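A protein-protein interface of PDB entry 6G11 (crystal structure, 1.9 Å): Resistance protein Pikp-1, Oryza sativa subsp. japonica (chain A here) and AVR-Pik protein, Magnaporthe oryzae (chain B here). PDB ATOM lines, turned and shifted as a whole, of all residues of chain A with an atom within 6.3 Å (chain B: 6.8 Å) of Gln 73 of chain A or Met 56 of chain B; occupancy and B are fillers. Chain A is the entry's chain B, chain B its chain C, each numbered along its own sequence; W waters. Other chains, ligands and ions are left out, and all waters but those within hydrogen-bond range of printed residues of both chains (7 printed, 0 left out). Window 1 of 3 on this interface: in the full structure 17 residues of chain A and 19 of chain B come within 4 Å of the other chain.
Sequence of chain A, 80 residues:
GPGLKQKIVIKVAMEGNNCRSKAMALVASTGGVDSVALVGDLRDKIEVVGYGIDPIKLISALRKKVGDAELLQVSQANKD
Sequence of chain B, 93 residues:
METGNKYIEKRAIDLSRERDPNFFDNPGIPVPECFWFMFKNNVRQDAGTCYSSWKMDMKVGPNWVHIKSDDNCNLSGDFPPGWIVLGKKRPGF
O of Leu 72 of chain A sits at hydrogen-bond distance from N of Lys 59 of chain B (2.8 Å). The side-chain amino group (NZ) of Lys 59 of chain B lies within salt-bridge range of the side-chain carboxylate (OE2) of Glu 70 of chain A. The backbone NH of Val 74 of chain A sits at hydrogen-bond distance from the backbone carbonyl oxygen of Asp 57 of chain B (3.2 Å).
The side-chain carboxylate (OD1) of Asp 57 of chain B is in hydrogen-bond range of a ring nitrogen (ND1) of His 66 of chain B, 2.6 Å away. The backbone NH (N) of Val 65 of chain B sits at hydrogen-bond distance from the backbone carbonyl oxygen (O) of Met 58 of chain B (2.8 Å). The backbone carbonyl oxygen (O) of Val 9 of chain A lies within hydrogen-bond range of the backbone NH (N) of Leu 72 of chain A. The backbone NH of Val 9 of chain A is in hydrogen-bond range of the backbone carbonyl oxygen of Gln 73 of chain A. O of Met 56 of chain B sits at hydrogen-bond distance from N of Ile 67 of chain B, at 2.8 Å.
Among the printed residues, merely in contact across the chains: Leu 72 of chain A with Met 58 of chain B, Gln 73 of chain A with Asp 57 of chain B, Gln 73 of chain A with Met 58 of chain B, Leu 71 of chain A with Trp 64 of chain B, Leu 72 of chain A with Trp 64 of chain B, Gln 73 of chain A with Trp 64 of chain B and Gln 73 of chain A with Met 56 of chain B.
Of the printed residues of chain B, Glu 70 of chain A touches Lys 59 (3.1 Å). Of chain B, only Met 56 (3.9 Å), Asp 57 (3.4 Å), Met 58 (3.5 Å) and Trp 64 (3.7 Å) come within 4 Å of Gln 73 of chain A. Trp 54 of chain B touches none of the printed residues of chain A. Of the printed residues of chain A, Met 56 of chain B touches Gln 73 (3.9 Å). Of the printed residues of chain A, Lys 59 of chain B touches Glu 70 (3.1 Å) and Leu 72 (2.8 Å). The nearest printed residue of chain A that does not touch Met 56 of chain B is Val 74 of chain A (4.7 Å).
Of the 11 printed residues of chain A, 5 touch a printed residue of chain B. Hydrophobic or aromatic side chains of chain B that line the printed part of chain A: Met 56, Met 58 and Trp 64.
Water W2 lies within hydrogen-bond range of the backbone carbonyl oxygen of Lys 55 of chain B (2.6 Å) and the side-chain hydroxyl of Ser 75 of chain A (3.2 Å). Water W1 lies within hydrogen-bond range of NE2 of Gln 73 of chain A (2.7 Å), O of Thr 49 of chain B (2.8 Å) and NZ of Lys 7 of chain A (2.9 Å). Water W7 lies within hydrogen-bond range of the side-chain hydroxyl (OG1) of Thr 49 of chain B (2.8 Å), the side-chain carboxylate (OE2) of Glu 47 of chain A (2.9 Å) and the side-chain amino group (NZ) of Lys 7 of chain A (3.1 Å). Water W3 bridges OH of Tyr 51 of chain B (2.8 Å) and NZ of Lys 7 of chain A (3.0 Å). Water W5 bridges O of Leu 71 of chain A (2.8 Å) and NZ of Lys 59 of chain B (2.9 Å). Water W6 lies within hydrogen-bond range of OE1 of Gln 73 of chain A (2.9 Å), O of Thr 49 of chain B (2.9 Å) and NE1 of Trp 36 of chain B (3.0 Å).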
ATOM      1  N   LYS A   7       3.997 -32.275  13.216  1.00  0.00           N
ATOM      2  CA  LYS A   7       4.734 -31.515  14.209  1.00  0.00           C
ATOM      3  C   LYS A   7       3.785 -31.237  15.352  1.00  0.00           C
ATOM      4  O   LYS A   7       2.671 -30.701  15.143  1.00  0.00           O
ATOM      5  CB  LYS A   7       5.255 -30.179  13.667  1.00  0.00           C
ATOM      6  CG  LYS A   7       6.078 -29.370  14.703  1.00  0.00           C
ATOM      7  CD  LYS A   7       6.315 -27.927  14.268  1.00  0.00           C
ATOM      8  CE  LYS A   7       7.156 -27.838  13.046  1.00  0.00           C
ATOM      9  NZ  LYS A   7       7.167 -26.415  12.531  1.00  0.00           N
ATOM     10  N   ILE A   8       4.204 -31.619  16.536  1.00  0.00           N
ATOM     11  CA  ILE A   8       3.417 -31.487  17.737  1.00  0.00           C
ATOM     12  C   ILE A   8       4.252 -30.734  18.759  1.00  0.00           C
ATOM     13  O   ILE A   8       5.441 -31.086  18.961  1.00  0.00           O
ATOM     14  CB  ILE A   8       3.074 -32.884  18.267  1.00  0.00           C
ATOM     15  CG1 ILE A   8       2.137 -33.611  17.290  1.00  0.00           C
ATOM     16  CG2 ILE A   8       2.438 -32.796  19.627  1.00  0.00           C
ATOM     17  CD1 ILE A   8       2.101 -35.113  17.470  1.00  0.00           C
ATOM     18  N   VAL A   9       3.651 -29.709  19.393  1.00  0.00           N
ATOM     19  CA  VAL A   9       4.341 -28.979  20.486  1.00  0.00           C
ATOM     20  C   VAL A   9       3.568 -29.142  21.795  1.00  0.00           C
ATOM     21  O   VAL A   9       2.347 -28.914  21.822  1.00  0.00           O
ATOM     22  CB  VAL A   9       4.568 -27.510  20.168  1.00  0.00           C
ATOM     23  CG1 VAL A   9       5.300 -26.812  21.285  1.00  0.00           C
ATOM     24  CG2 VAL A   9       5.353 -27.338  18.877  1.00  0.00           C
ATOM     25  N   ILE A  10       4.260 -29.578  22.843  1.00  0.00           N
ATOM     26  CA  ILE A  10       3.661 -29.826  24.146  1.00  0.00           C
ATOM     27  C   ILE A  10       4.389 -29.040  25.238  1.00  0.00           C
ATOM     28  O   ILE A  10       5.598 -29.079  25.314  1.00  0.00           O
ATOM     29  CB  ILE A  10       3.750 -31.307  24.484  1.00  0.00           C
ATOM     30  CG1 ILE A  10       2.906 -32.098  23.455  1.00  0.00           C
ATOM     31  CG2 ILE A  10       3.254 -31.576  25.906  1.00  0.00           C
ATOM     32  CD1 ILE A  10       2.976 -33.599  23.590  1.00  0.00           C
ATOM     33  N   GLU A  47       9.019 -29.983  21.200  1.00  0.00           N
ATOM     34  CA  GLU A  47       8.627 -30.035  19.808  1.00  0.00           C
ATOM     35  C   GLU A  47       9.012 -31.409  19.251  1.00  0.00           C
ATOM     36  O   GLU A  47      10.192 -31.785  19.294  1.00  0.00           O
ATOM     37  CB  GLU A  47       9.288 -28.893  19.015  1.00  0.00           C
ATOM     38  CG  GLU A  47       8.868 -28.921  17.566  1.00  0.00           C
ATOM     39  CD  GLU A  47       9.354 -27.720  16.751  1.00  0.00           C
ATOM     40  OE1 GLU A  47       9.893 -27.976  15.654  1.00  0.00           O
ATOM     41  OE2 GLU A  47       9.229 -26.555  17.154  1.00  0.00           O
ATOM     42  N   GLU A  70       0.356 -29.826  28.430  1.00  0.00           N
ATOM     43  CA  GLU A  70      -0.679 -29.177  27.653  1.00  0.00           C
ATOM     44  C   GLU A  70      -0.278 -29.214  26.176  1.00  0.00           C
ATOM     45  O   GLU A  70       0.858 -28.887  25.819  1.00  0.00           O
ATOM     46  CB  GLU A  70      -0.793 -27.726  28.116  1.00  0.00           C
ATOM     47  CG  GLU A  70      -2.033 -26.942  27.697  1.00  0.00           C
ATOM     48  CD  GLU A  70      -1.880 -25.413  27.799  1.00  0.00           C
ATOM     49  OE1 GLU A  70      -0.895 -24.923  28.415  1.00  0.00           O
ATOM     50  OE2 GLU A  70      -2.732 -24.673  27.240  1.00  0.00           O
ATOM     51  N   LEU A  71      -1.213 -29.614  25.324  1.00  0.00           N
ATOM     52  CA  LEU A  71      -0.967 -29.617  23.889  1.00  0.00           C
ATOM     53  C   LEU A  71      -1.081 -28.183  23.379  1.00  0.00           C
ATOM     54  O   LEU A  71      -2.090 -27.525  23.619  1.00  0.00           O
ATOM     55  CB  LEU A  71      -2.002 -30.488  23.229  1.00  0.00           C
ATOM     56  CG  LEU A  71      -1.827 -30.831  21.778  1.00  0.00           C
ATOM     57  CD1 LEU A  71      -0.505 -31.516  21.499  1.00  0.00           C
ATOM     58  CD2 LEU A  71      -2.982 -31.756  21.385  1.00  0.00           C
ATOM     59  N   LEU A  72      -0.054 -27.687  22.704  1.00  0.00           N
ATOM     60  CA  LEU A  72      -0.051 -26.321  22.215  1.00  0.00           C
ATOM     61  C   LEU A  72      -0.130 -26.153  20.715  1.00  0.00           C
ATOM     62  O   LEU A  72      -0.552 -25.085  20.258  1.00  0.00           O
ATOM     63  CB  LEU A  72       1.199 -25.608  22.704  1.00  0.00           C
ATOM     64  CG  LEU A  72       1.358 -25.379  24.188  1.00  0.00           C
ATOM     65  CD1 LEU A  72       2.608 -24.537  24.403  1.00  0.00           C
ATOM     66  CD2 LEU A  72       0.168 -24.691  24.821  1.00  0.00           C
ATOM     67  N   GLN A  73       0.335 -27.145  19.953  1.00  0.00           N
ATOM     68  CA  GLN A  73       0.421 -26.973  18.504  1.00  0.00           C
ATOM     69  C   GLN A  73       0.379 -28.351  17.871  1.00  0.00           C
ATOM     70  O   GLN A  73       1.000 -29.316  18.371  1.00  0.00           O
ATOM     71  CB  GLN A  73       1.691 -26.246  18.094  1.00  0.00           C
ATOM     72  CG  GLN A  73       1.725 -25.817  16.675  1.00  0.00           C
ATOM     73  CD  GLN A  73       3.037 -25.154  16.259  1.00  0.00           C
ATOM     74  OE1 GLN A  73       3.669 -24.405  17.040  1.00  0.00           O
ATOM     75  NE2 GLN A  73       3.482 -25.463  15.018  1.00  0.00           N
ATOM     76  N   VAL A  74      -0.382 -28.448  16.783  1.00  0.00           N
ATOM     77  CA  VAL A  74      -0.442 -29.632  15.954  1.00  0.00           C
ATOM     78  C   VAL A  74      -0.468 -29.147  14.520  1.00  0.00           C
ATOM     79  O   VAL A  74      -1.269 -28.283  14.150  1.00  0.00           O
ATOM     80  CB  VAL A  74      -1.709 -30.456  16.212  1.00  0.00           C
ATOM     81  CG1 VAL A  74      -1.844 -31.615  15.224  1.00  0.00           C
ATOM     82  CG2 VAL A  74      -1.711 -31.011  17.643  1.00  0.00           C
ATOM     83  N   SER A  75       0.443 -29.718  13.708  1.00  0.00           N
ATOM     84  CA  SER A  75       0.261 -29.904  12.270  1.00  0.00           C
ATOM     85  C   SER A  75       0.330 -31.431  11.963  1.00  0.00           C
ATOM     86  O   SER A  75       1.240 -32.089  12.445  1.00  0.00           O
ATOM     87  CB  SER A  75       1.404 -29.201  11.552  1.00  0.00           C
ATOM     88  OG  SER A  75       1.483 -29.553  10.189  1.00  0.00           O
ATOM     89  N   TRP B  36       7.524 -16.712  14.694  1.00  0.00           N
ATOM     90  CA  TRP B  36       6.278 -16.163  15.205  1.00  0.00           C
ATOM     91  C   TRP B  36       6.465 -15.797  16.658  1.00  0.00           C
ATOM     92  O   TRP B  36       7.261 -16.418  17.370  1.00  0.00           O
ATOM     93  CB  TRP B  36       5.069 -17.110  15.046  1.00  0.00           C
ATOM     94  CG  TRP B  36       5.222 -18.421  15.730  1.00  0.00           C
ATOM     95  CD1 TRP B  36       5.612 -19.583  15.140  1.00  0.00           C
ATOM     96  CD2 TRP B  36       5.011 -18.724  17.119  1.00  0.00           C
ATOM     97  NE1 TRP B  36       5.656 -20.597  16.071  1.00  0.00           N
ATOM     98  CE2 TRP B  36       5.305 -20.091  17.294  1.00  0.00           C
ATOM     99  CE3 TRP B  36       4.605 -17.972  18.234  1.00  0.00           C
ATOM    100  CZ2 TRP B  36       5.209 -20.742  18.553  1.00  0.00           C
ATOM    101  CZ3 TRP B  36       4.504 -18.611  19.483  1.00  0.00           C
ATOM    102  CH2 TRP B  36       4.803 -19.990  19.620  1.00  0.00           C
ATOM    103  N   GLY B  48       8.242 -19.063  18.339  1.00  0.00           N
ATOM    104  CA  GLY B  48       8.737 -20.268  17.694  1.00  0.00           C
ATOM    105  C   GLY B  48       8.915 -20.040  16.207  1.00  0.00           C
ATOM    106  O   GLY B  48       9.039 -18.893  15.761  1.00  0.00           O
ATOM    107  N   THR B  49       8.862 -21.133  15.441  1.00  0.00           N
ATOM    108  CA  THR B  49       9.026 -21.066  13.970  1.00  0.00           C
ATOM    109  C   THR B  49       7.775 -21.631  13.282  1.00  0.00           C
ATOM    110  O   THR B  49       7.013 -22.437  13.861  1.00  0.00           O
ATOM    111  CB  THR B  49      10.272 -21.851  13.506  1.00  0.00           C
ATOM    112  OG1 THR B  49      10.105 -23.220  13.854  1.00  0.00           O
ATOM    113  CG2 THR B  49      11.565 -21.352  14.125  1.00  0.00           C
ATOM    114  N   CYS B  50       7.553 -21.206  12.050  1.00  0.00           N
ATOM    115  CA  CYS B  50       6.502 -21.750  11.213  1.00  0.00           C
ATOM    116  C   CYS B  50       6.814 -21.481   9.745  1.00  0.00           C
ATOM    117  O   CYS B  50       7.651 -20.620   9.415  1.00  0.00           O
ATOM    118  CB  CYS B  50       5.125 -21.157  11.558  1.00  0.00           C
ATOM    119  SG  CYS B  50       4.953 -19.375  11.255  1.00  0.00           S
ATOM    120  N   TYR B  51       6.157 -22.245   8.873  1.00  0.00           N
ATOM    121  CA  TYR B  51       6.325 -22.079   7.421  1.00  0.00           C
ATOM    122  C   TYR B  51       5.603 -20.861   6.892  1.00  0.00           C
ATOM    123  O   TYR B  51       4.542 -20.492   7.404  1.00  0.00           O
ATOM    124  CB  TYR B  51       5.800 -23.308   6.684  1.00  0.00           C
ATOM    125  CG  TYR B  51       6.630 -24.538   6.915  1.00  0.00           C
ATOM    126  CD1 TYR B  51       7.894 -24.652   6.343  1.00  0.00           C
ATOM    127  CD2 TYR B  51       6.141 -25.609   7.704  1.00  0.00           C
ATOM    128  CE1 TYR B  51       8.675 -25.786   6.539  1.00  0.00           C
ATOM    129  CE2 TYR B  51       6.897 -26.743   7.913  1.00  0.00           C
ATOM    130  CZ  TYR B  51       8.163 -26.834   7.342  1.00  0.00           C
ATOM    131  OH  TYR B  51       8.929 -27.944   7.554  1.00  0.00           O
ATOM    132  N   TRP B  54       1.484 -20.930   4.482  1.00  0.00           N
ATOM    133  CA  TRP B  54       1.089 -22.178   5.117  1.00  0.00           C
ATOM    134  C   TRP B  54       0.099 -21.886   6.223  1.00  0.00           C
ATOM    135  O   TRP B  54      -0.569 -20.871   6.186  1.00  0.00           O
ATOM    136  CB  TRP B  54       2.336 -22.917   5.612  1.00  0.00           C
ATOM    137  CG  TRP B  54       2.175 -24.422   5.806  1.00  0.00           C
ATOM    138  CD1 TRP B  54       2.457 -25.155   6.951  1.00  0.00           C
ATOM    139  CD2 TRP B  54       1.716 -25.374   4.824  1.00  0.00           C
ATOM    140  NE1 TRP B  54       2.179 -26.500   6.730  1.00  0.00           N
ATOM    141  CE2 TRP B  54       1.726 -26.659   5.441  1.00  0.00           C
ATOM    142  CE3 TRP B  54       1.287 -25.261   3.480  1.00  0.00           C
ATOM    143  CZ2 TRP B  54       1.330 -27.826   4.759  1.00  0.00           C
ATOM    144  CZ3 TRP B  54       0.899 -26.409   2.795  1.00  0.00           C
ATOM    145  CH2 TRP B  54       0.931 -27.690   3.441  1.00  0.00           C
ATOM    146  N   LYS B  55      -0.043 -22.805   7.168  1.00  0.00           N
ATOM    147  CA  LYS B  55      -1.091 -22.740   8.184  1.00  0.00           C
ATOM    148  C   LYS B  55      -0.652 -23.641   9.351  1.00  0.00           C
ATOM    149  O   LYS B  55       0.132 -24.597   9.171  1.00  0.00           O
ATOM    150  CB  LYS B  55      -2.415 -23.234   7.607  1.00  0.00           C
ATOM    151  CG  LYS B  55      -2.379 -24.727   7.210  1.00  0.00           C
ATOM    152  CD  LYS B  55      -3.026 -25.025   5.884  1.00  0.00           C
ATOM    153  CE  LYS B  55      -2.859 -26.498   5.528  1.00  0.00           C
ATOM    154  NZ  LYS B  55      -1.672 -26.739   4.704  1.00  0.00           N
ATOM    155  N   MET B  56      -1.135 -23.299  10.534  1.00  0.00           N
ATOM    156  CA  MET B  56      -0.899 -24.096  11.732  1.00  0.00           C
ATOM    157  C   MET B  56      -2.026 -23.860  12.729  1.00  0.00           C
ATOM    158  O   MET B  56      -2.671 -22.787  12.725  1.00  0.00           O
ATOM    159  CB  MET B  56       0.470 -23.790  12.354  1.00  0.00           C
ATOM    160  CG  MET B  56       0.671 -22.388  12.885  1.00  0.00           C
ATOM    161  SD  MET B  56       2.213 -21.944  13.783  1.00  0.00           S
ATOM    162  CE  MET B  56       2.038 -20.172  13.572  1.00  0.00           C
ATOM    163  N   ASP B  57      -2.247 -24.859  13.594  1.00  0.00           N
ATOM    164  CA  ASP B  57      -3.242 -24.782  14.621  1.00  0.00           C
ATOM    165  C   ASP B  57      -2.508 -24.692  15.931  1.00  0.00           C
ATOM    166  O   ASP B  57      -1.671 -25.526  16.227  1.00  0.00           O
ATOM    167  CB  ASP B  57      -4.179 -25.997  14.577  1.00  0.00           C
ATOM    168  CG  ASP B  57      -5.052 -25.999  13.348  1.00  0.00           C
ATOM    169  OD1 ASP B  57      -5.556 -24.938  12.905  1.00  0.00           O
ATOM    170  OD2 ASP B  57      -5.193 -27.091  12.775  1.00  0.00           O
ATOM    171  N   MET B  58      -2.810 -23.633  16.678  1.00  0.00           N
ATOM    172  CA  MET B  58      -2.054 -23.262  17.876  1.00  0.00           C
ATOM    173  C   MET B  58      -3.005 -22.824  18.937  1.00  0.00           C
ATOM    174  O   MET B  58      -3.968 -22.069  18.665  1.00  0.00           O
ATOM    175  CB  MET B  58      -1.130 -22.082  17.560  1.00  0.00           C
ATOM    176  CG  MET B  58      -0.222 -21.685  18.736  1.00  0.00           C
ATOM    177  SD  MET B  58       0.939 -20.350  18.315  1.00  0.00           S
ATOM    178  CE  MET B  58       2.059 -21.315  17.345  1.00  0.00           C
ATOM    179  N   LYS B  59      -2.713 -23.260  20.139  1.00  0.00           N
ATOM    180  CA  LYS B  59      -3.418 -22.844  21.318  1.00  0.00           C
ATOM    181  C   LYS B  59      -2.937 -21.433  21.683  1.00  0.00           C
ATOM    182  O   LYS B  59      -1.743 -21.231  21.963  1.00  0.00           O
ATOM    183  CB  LYS B  59      -3.118 -23.824  22.422  1.00  0.00           C
ATOM    184  CG  LYS B  59      -3.923 -23.668  23.693  1.00  0.00           C
ATOM    185  CD  LYS B  59      -5.315 -24.229  23.579  1.00  0.00           C
ATOM    186  CE  LYS B  59      -5.978 -24.291  24.950  1.00  0.00           C
ATOM    187  NZ  LYS B  59      -5.355 -25.332  25.814  1.00  0.00           N
ATOM    188  N   TRP B  64      -7.979 -22.757  20.626  1.00  0.00           N
ATOM    189  CA  TRP B  64      -7.259 -23.165  19.437  1.00  0.00           C
ATOM    190  C   TRP B  64      -7.549 -22.187  18.330  1.00  0.00           C
ATOM    191  O   TRP B  64      -8.690 -21.803  18.152  1.00  0.00           O
ATOM    192  CB  TRP B  64      -7.652 -24.555  19.003  1.00  0.00           C
ATOM    193  CG  TRP B  64      -7.028 -25.561  19.854  1.00  0.00           C
ATOM    194  CD1 TRP B  64      -7.563 -26.155  20.958  1.00  0.00           C
ATOM    195  CD2 TRP B  64      -5.705 -26.086  19.701  1.00  0.00           C
ATOM    196  NE1 TRP B  64      -6.638 -27.039  21.515  1.00  0.00           N
ATOM    197  CE2 TRP B  64      -5.502 -27.031  20.740  1.00  0.00           C
ATOM    198  CE3 TRP B  64      -4.689 -25.872  18.772  1.00  0.00           C
ATOM    199  CZ2 TRP B  64      -4.328 -27.738  20.880  1.00  0.00           C
ATOM    200  CZ3 TRP B  64      -3.509 -26.569  18.926  1.00  0.00           C
ATOM    201  CH2 TRP B  64      -3.339 -27.503  19.964  1.00  0.00           C
ATOM    202  N   VAL B  65      -6.529 -21.782  17.600  1.00  0.00           N
ATOM    203  CA  VAL B  65      -6.695 -20.830  16.537  1.00  0.00           C
ATOM    204  C   VAL B  65      -6.013 -21.400  15.296  1.00  0.00           C
ATOM    205  O   VAL B  65      -4.843 -21.814  15.371  1.00  0.00           O
ATOM    206  CB  VAL B  65      -6.044 -19.470  16.884  1.00  0.00           C
ATOM    207  CG1 VAL B  65      -6.209 -18.477  15.710  1.00  0.00           C
ATOM    208  CG2 VAL B  65      -6.605 -18.895  18.158  1.00  0.00           C
ATOM    209  N   HIS B  66      -6.685 -21.315  14.156  1.00  0.00           N
ATOM    210  CA  HIS B  66      -6.116 -21.683  12.871  1.00  0.00           C
ATOM    211  C   HIS B  66      -5.435 -20.424  12.346  1.00  0.00           C
ATOM    212  O   HIS B  66      -6.104 -19.421  12.052  1.00  0.00           O
ATOM    213  CB  HIS B  66      -7.221 -22.175  11.903  1.00  0.00           C
ATOM    214  CG  HIS B  66      -6.704 -22.734  10.613  1.00  0.00           C
ATOM    215  ND1 HIS B  66      -6.129 -23.993  10.513  1.00  0.00           N
ATOM    216  CD2 HIS B  66      -6.690 -22.209   9.359  1.00  0.00           C
ATOM    217  CE1 HIS B  66      -5.740 -24.192   9.259  1.00  0.00           C
ATOM    218  NE2 HIS B  66      -6.094 -23.137   8.531  1.00  0.00           N
ATOM    219  N   ILE B  67      -4.110 -20.466  12.261  1.00  0.00           N
ATOM    220  CA  ILE B  67      -3.320 -19.298  11.861  1.00  0.00           C
ATOM    221  C   ILE B  67      -2.726 -19.565  10.492  1.00  0.00           C
ATOM    222  O   ILE B  67      -2.046 -20.581  10.319  1.00  0.00           O
ATOM    223  CB  ILE B  67      -2.165 -19.030  12.846  1.00  0.00           C
ATOM    224  CG1 ILE B  67      -2.702 -18.891  14.268  1.00  0.00           C
ATOM    225  CG2 ILE B  67      -1.376 -17.790  12.383  1.00  0.00           C
ATOM    226  CD1 ILE B  67      -1.587 -18.797  15.312  1.00  0.00           C
ATOM    227  N   LYS B  68      -2.996 -18.670   9.545  1.00  0.00           N
ATOM    228  CA  LYS B  68      -2.411 -18.707   8.204  1.00  0.00           C
ATOM    229  C   LYS B  68      -1.263 -17.735   8.033  1.00  0.00           C
ATOM    230  O   LYS B  68      -1.283 -16.656   8.590  1.00  0.00           O
ATOM    231  CB  LYS B  68      -3.490 -18.377   7.173  1.00  0.00           C
ATOM    232  CG  LYS B  68      -4.487 -19.527   7.029  1.00  0.00           C
ATOM    233  CD  LYS B  68      -5.356 -19.396   5.791  1.00  0.00           C
ATOM    234  CE  LYS B  68      -6.417 -18.332   5.983  1.00  0.00           C
ATOM    235  NZ  LYS B  68      -7.654 -18.725   5.230  1.00  0.00           N
ATOM    236  N   SER B  69      -0.276 -18.135   7.242  1.00  0.00           N
ATOM    237  CA  SER B  69       0.853 -17.319   6.931  1.00  0.00           C
ATOM    238  C   SER B  69       0.872 -17.064   5.421  1.00  0.00           C
ATOM    239  O   SER B  69       0.574 -17.963   4.622  1.00  0.00           O
ATOM    240  CB  SER B  69       2.131 -18.034   7.382  1.00  0.00           C
ATOM    241  OG  SER B  69       2.363 -19.194   6.617  1.00  0.00           O
ATOM    242  N   LEU B  75       0.983 -13.131   9.519  1.00  0.00           N
ATOM    243  CA  LEU B  75       0.128 -14.166  10.043  1.00  0.00           C
ATOM    244  C   LEU B  75      -1.287 -13.604  10.247  1.00  0.00           C
ATOM    245  O   LEU B  75      -1.463 -12.451  10.655  1.00  0.00           O
ATOM    246  CB  LEU B  75       0.683 -14.631  11.366  1.00  0.00           C
ATOM    247  CG  LEU B  75       2.116 -15.182  11.335  1.00  0.00           C
ATOM    248  CD1 LEU B  75       2.530 -15.604  12.746  1.00  0.00           C
ATOM    249  CD2 LEU B  75       2.243 -16.343  10.371  1.00  0.00           C
ATOM    250  N   VAL B  85      -0.714 -13.111  17.501  1.00  0.00           N
ATOM    251  CA  VAL B  85       0.491 -13.789  17.030  1.00  0.00           C
ATOM    252  C   VAL B  85       0.951 -13.097  15.762  1.00  0.00           C
ATOM    253  O   VAL B  85       0.160 -12.921  14.811  1.00  0.00           O
ATOM    254  CB  VAL B  85       0.280 -15.266  16.768  1.00  0.00           C
ATOM    255  CG1 VAL B  85       1.613 -15.939  16.419  1.00  0.00           C
ATOM    256  CG2 VAL B  85      -0.319 -15.949  18.023  1.00  0.00           C
HETATM  257  O   HOH W   1       5.128 -24.414  13.198  1.00  0.00           O
HETATM  258  O   HOH W   2      -0.295 -27.149   9.188  1.00  0.00           O
HETATM  259  O   HOH W   3       8.719 -27.803  10.322  1.00  0.00           O
HETATM  260  O   HOH W   4      -3.727 -29.441  12.936  1.00  0.00           O
HETATM  261  O   HOH W   5      -4.457 -27.948  25.015  1.00  0.00           O
HETATM  262  O   HOH W   6       6.328 -23.511  16.515  1.00  0.00           O
HETATM  263  O   HOH W   7       8.240 -24.904  14.985  1.00  0.00           O
